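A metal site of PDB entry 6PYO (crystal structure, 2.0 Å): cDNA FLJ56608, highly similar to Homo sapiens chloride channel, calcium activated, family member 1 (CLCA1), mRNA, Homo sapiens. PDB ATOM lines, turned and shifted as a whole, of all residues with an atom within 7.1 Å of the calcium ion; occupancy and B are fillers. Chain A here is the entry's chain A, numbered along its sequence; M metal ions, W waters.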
ATOM      1  N   ASP A  14     -21.624  15.633 -14.945  1.00  0.00           N
ATOM      2  CA  ASP A  14     -22.375  14.615 -15.678  1.00  0.00           C
ATOM      3  C   ASP A  14     -21.696  14.342 -17.015  1.00  0.00           C
ATOM      4  O   ASP A  14     -21.635  15.228 -17.879  1.00  0.00           O
ATOM      5  CB  ASP A  14     -23.794  15.145 -15.848  1.00  0.00           C
ATOM      6  CG  ASP A  14     -24.758  14.115 -16.406  1.00  0.00           C
ATOM      7  OD1 ASP A  14     -24.296  13.147 -17.068  1.00  0.00           O
ATOM      8  OD2 ASP A  14     -25.969  14.318 -16.188  1.00  0.00           O
ATOM      9  N   LYS A  15     -21.129  13.132 -17.174  1.00  0.00           N
ATOM     10  CA  LYS A  15     -20.578  12.704 -18.448  1.00  0.00           C
ATOM     11  C   LYS A  15     -21.409  11.586 -19.088  1.00  0.00           C
ATOM     12  O   LYS A  15     -20.872  10.810 -19.901  1.00  0.00           O
ATOM     13  CB  LYS A  15     -19.103  12.278 -18.311  1.00  0.00           C
ATOM     14  CG  LYS A  15     -18.888  11.147 -17.295  1.00  0.00           C
ATOM     15  CD  LYS A  15     -17.846  10.137 -17.708  1.00  0.00           C
ATOM     16  CE  LYS A  15     -18.091   9.527 -19.083  1.00  0.00           C
ATOM     17  NZ  LYS A  15     -18.960   8.316 -19.018  1.00  0.00           N
ATOM     18  N   SER A  16     -22.683  11.466 -18.727  1.00  0.00           N
ATOM     19  CA  SER A  16     -23.534  10.371 -19.195  1.00  0.00           C
ATOM     20  C   SER A  16     -23.868  10.547 -20.675  1.00  0.00           C
ATOM     21  O   SER A  16     -23.614  11.591 -21.267  1.00  0.00           O
ATOM     22  CB  SER A  16     -24.809  10.303 -18.353  1.00  0.00           C
ATOM     23  OG  SER A  16     -25.629  11.453 -18.499  1.00  0.00           O
ATOM     24  N   GLY A  17     -24.484   9.513 -21.260  1.00  0.00           N
ATOM     25  CA  GLY A  17     -24.721   9.527 -22.701  1.00  0.00           C
ATOM     26  C   GLY A  17     -25.623  10.656 -23.156  1.00  0.00           C
ATOM     27  O   GLY A  17     -25.423  11.200 -24.258  1.00  0.00           O
ATOM     28  N   SER A  18     -26.635  11.018 -22.356  1.00  0.00           N
ATOM     29  CA  SER A  18     -27.504  12.134 -22.728  1.00  0.00           C
ATOM     30  C   SER A  18     -26.704  13.403 -22.948  1.00  0.00           C
ATOM     31  O   SER A  18     -27.140  14.271 -23.711  1.00  0.00           O
ATOM     32  CB  SER A  18     -28.579  12.404 -21.673  1.00  0.00           C
ATOM     33  OG  SER A  18     -28.042  12.574 -20.364  1.00  0.00           O
ATOM     34  N   MET A  19     -25.582  13.547 -22.255  1.00  0.00           N
ATOM     35  CA  MET A  19     -24.775  14.756 -22.385  1.00  0.00           C
ATOM     36  C   MET A  19     -24.152  14.883 -23.767  1.00  0.00           C
ATOM     37  O   MET A  19     -23.665  15.959 -24.112  1.00  0.00           O
ATOM     38  CB  MET A  19     -23.700  14.767 -21.288  1.00  0.00           C
ATOM     39  CG  MET A  19     -24.293  14.928 -19.896  1.00  0.00           C
ATOM     40  SD  MET A  19     -25.073  16.569 -19.652  1.00  0.00           S
ATOM     41  CE  MET A  19     -23.580  17.541 -19.486  1.00  0.00           C
ATOM     42  N   ARG A  24     -24.201  19.983 -25.007  1.00  0.00           N
ATOM     43  CA  ARG A  24     -24.277  19.959 -23.561  1.00  0.00           C
ATOM     44  C   ARG A  24     -22.910  19.750 -22.949  1.00  0.00           C
ATOM     45  O   ARG A  24     -22.563  20.406 -21.966  1.00  0.00           O
ATOM     46  CB  ARG A  24     -25.226  18.861 -23.095  1.00  0.00           C
ATOM     47  CG  ARG A  24     -26.627  19.075 -23.572  1.00  0.00           C
ATOM     48  CD  ARG A  24     -27.490  17.905 -23.216  1.00  0.00           C
ATOM     49  NE  ARG A  24     -28.826  18.090 -23.744  1.00  0.00           N
ATOM     50  CZ  ARG A  24     -29.874  17.346 -23.415  1.00  0.00           C
ATOM     51  NH1 ARG A  24     -29.780  16.351 -22.547  1.00  0.00           N
ATOM     52  NH2 ARG A  24     -31.043  17.642 -23.956  1.00  0.00           N
ATOM     53  N   PHE A  51     -19.448  11.536 -13.428  1.00  0.00           N
ATOM     54  CA  PHE A  51     -20.312  10.417 -13.133  1.00  0.00           C
ATOM     55  C   PHE A  51     -21.063  10.052 -14.407  1.00  0.00           C
ATOM     56  O   PHE A  51     -21.405  10.928 -15.208  1.00  0.00           O
ATOM     57  CB  PHE A  51     -21.285  10.695 -11.982  1.00  0.00           C
ATOM     58  CG  PHE A  51     -22.320  11.720 -12.309  1.00  0.00           C
ATOM     59  CD1 PHE A  51     -23.542  11.347 -12.887  1.00  0.00           C
ATOM     60  CD2 PHE A  51     -22.085  13.053 -12.043  1.00  0.00           C
ATOM     61  CE1 PHE A  51     -24.493  12.312 -13.188  1.00  0.00           C
ATOM     62  CE2 PHE A  51     -23.012  14.024 -12.340  1.00  0.00           C
ATOM     63  CZ  PHE A  51     -24.228  13.660 -12.899  1.00  0.00           C
ATOM     64  N   GLY A  83     -22.601   6.254 -21.194  1.00  0.00           N
ATOM     65  CA  GLY A  83     -22.997   5.533 -20.000  1.00  0.00           C
ATOM     66  C   GLY A  83     -24.306   6.062 -19.464  1.00  0.00           C
ATOM     67  O   GLY A  83     -24.942   6.956 -20.023  1.00  0.00           O
ATOM     68  N   GLY A  84     -24.720   5.464 -18.354  1.00  0.00           N
ATOM     69  CA  GLY A  84     -25.975   5.836 -17.744  1.00  0.00           C
ATOM     70  C   GLY A  84     -25.793   6.996 -16.792  1.00  0.00           C
ATOM     71  O   GLY A  84     -24.729   7.609 -16.682  1.00  0.00           O
ATOM     72  N   THR A  85     -26.871   7.286 -16.079  1.00  0.00           N
ATOM     73  CA  THR A  85     -26.992   8.494 -15.288  1.00  0.00           C
ATOM     74  C   THR A  85     -27.293   8.125 -13.851  1.00  0.00           C
ATOM     75  O   THR A  85     -28.279   7.423 -13.580  1.00  0.00           O
ATOM     76  CB  THR A  85     -28.095   9.386 -15.829  1.00  0.00           C
ATOM     77  OG1 THR A  85     -27.821   9.718 -17.198  1.00  0.00           O
ATOM     78  CG2 THR A  85     -28.129  10.694 -14.998  1.00  0.00           C
ATOM     79  N   SER A  86     -26.471   8.641 -12.904  1.00  0.00           N
ATOM     80  CA  SER A  86     -26.820   8.590 -11.484  1.00  0.00           C
ATOM     81  C   SER A  86     -26.255   9.842 -10.805  1.00  0.00           C
ATOM     82  O   SER A  86     -25.111   9.862 -10.341  1.00  0.00           O
ATOM     83  CB  SER A  86     -26.332   7.312 -10.832  1.00  0.00           C
ATOM     84  OG  SER A  86     -26.636   7.306  -9.455  1.00  0.00           O
ATOM     85  N   THR A 113     -25.163  19.332 -14.950  1.00  0.00           N
ATOM     86  CA  THR A 113     -25.850  18.166 -15.508  1.00  0.00           C
ATOM     87  C   THR A 113     -26.994  18.618 -16.394  1.00  0.00           C
ATOM     88  O   THR A 113     -27.509  19.732 -16.233  1.00  0.00           O
ATOM     89  CB  THR A 113     -26.415  17.265 -14.386  1.00  0.00           C
ATOM     90  OG1 THR A 113     -27.154  16.155 -14.928  1.00  0.00           O
ATOM     91  CG2 THR A 113     -27.384  18.095 -13.531  1.00  0.00           C
ATOM     92  N   ASP A 114     -27.427  17.711 -17.309  1.00  0.00           N
ATOM     93  CA  ASP A 114     -28.680  17.966 -18.014  1.00  0.00           C
ATOM     94  C   ASP A 114     -29.896  17.639 -17.146  1.00  0.00           C
ATOM     95  O   ASP A 114     -31.029  17.991 -17.518  1.00  0.00           O
ATOM     96  CB  ASP A 114     -28.768  17.215 -19.365  1.00  0.00           C
ATOM     97  CG  ASP A 114     -28.678  15.703 -19.262  1.00  0.00           C
ATOM     98  OD1 ASP A 114     -29.041  15.078 -18.251  1.00  0.00           O
ATOM     99  OD2 ASP A 114     -28.221  15.127 -20.253  1.00  0.00           O
ATOM    100  N   GLY A 115     -29.706  16.995 -15.992  1.00  0.00           N
ATOM    101  CA  GLY A 115     -30.792  16.753 -15.075  1.00  0.00           C
ATOM    102  C   GLY A 115     -31.763  15.653 -15.446  1.00  0.00           C
ATOM    103  O   GLY A 115     -32.758  15.479 -14.751  1.00  0.00           O
ATOM    104  N   GLU A 116     -31.460  14.875 -16.483  1.00  0.00           N
ATOM    105  CA  GLU A 116     -32.360  13.817 -16.956  1.00  0.00           C
ATOM    106  C   GLU A 116     -32.122  12.561 -16.128  1.00  0.00           C
ATOM    107  O   GLU A 116     -31.514  11.586 -16.571  1.00  0.00           O
ATOM    108  CB  GLU A 116     -32.129  13.590 -18.445  1.00  0.00           C
ATOM    109  CG  GLU A 116     -32.521  14.815 -19.210  1.00  0.00           C
ATOM    110  CD  GLU A 116     -32.149  14.772 -20.660  1.00  0.00           C
ATOM    111  OE1 GLU A 116     -31.618  13.726 -21.084  1.00  0.00           O
ATOM    112  OE2 GLU A 116     -32.385  15.786 -21.372  1.00  0.00           O
ATOM    113  N   ASP A 117     -32.643  12.602 -14.905  1.00  0.00           N
ATOM    114  CA  ASP A 117     -32.462  11.555 -13.897  1.00  0.00           C
ATOM    115  C   ASP A 117     -33.668  11.590 -12.969  1.00  0.00           C
ATOM    116  O   ASP A 117     -33.937  12.624 -12.360  1.00  0.00           O
ATOM    117  CB  ASP A 117     -31.176  11.800 -13.113  1.00  0.00           C
ATOM    118  CG  ASP A 117     -30.898  10.722 -12.082  1.00  0.00           C
ATOM    119  OD1 ASP A 117     -31.731   9.799 -11.873  1.00  0.00           O
ATOM    120  OD2 ASP A 117     -29.814  10.820 -11.463  1.00  0.00           O
HETATM  121 CA    CA M   1     -27.963  11.282 -18.659  1.00  0.00          CA
HETATM  122  O   HOH W   1     -27.969  13.194 -17.275  1.00  0.00           O
HETATM  123  O   HOH W   2     -30.325  10.832 -18.725  1.00  0.00           O
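The calcium ion is bound by the side-chain hydroxyl of Ser 18, the side-chain hydroxyl of Thr 85, the side-chain hydroxyl of Ser 16, water W1 and water W2.
The side-chain carboxylate (OD2) of Asp 114 sits close to the side-chain hydroxyl (OG) of Ser 18, at 2.6 Å.
The side-chain carboxylate of Asp 14 is in hydrogen-bond range of the backbone NH of Ser 16, at 2.9 Å.
The backbone NH (N) of Glu 116 is in hydrogen-bond range of the side-chain carboxylate (OD1) of Asp 114 (3.0 Å).
The backbone NH of Asp 114 lies within hydrogen-bond range of the side-chain sulfur of Met 19 (3.5 Å).
The side-chain carboxylate (OD2) of Asp 114 is in salt-bridge range of the guanidinium group (NH1) of Arg 24, at 3.0 Å.
Merely in contact with the calcium ion: Asp 114.
The nearest printed residue that does not touch the calcium ion is Glu 116 (4.1 Å).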
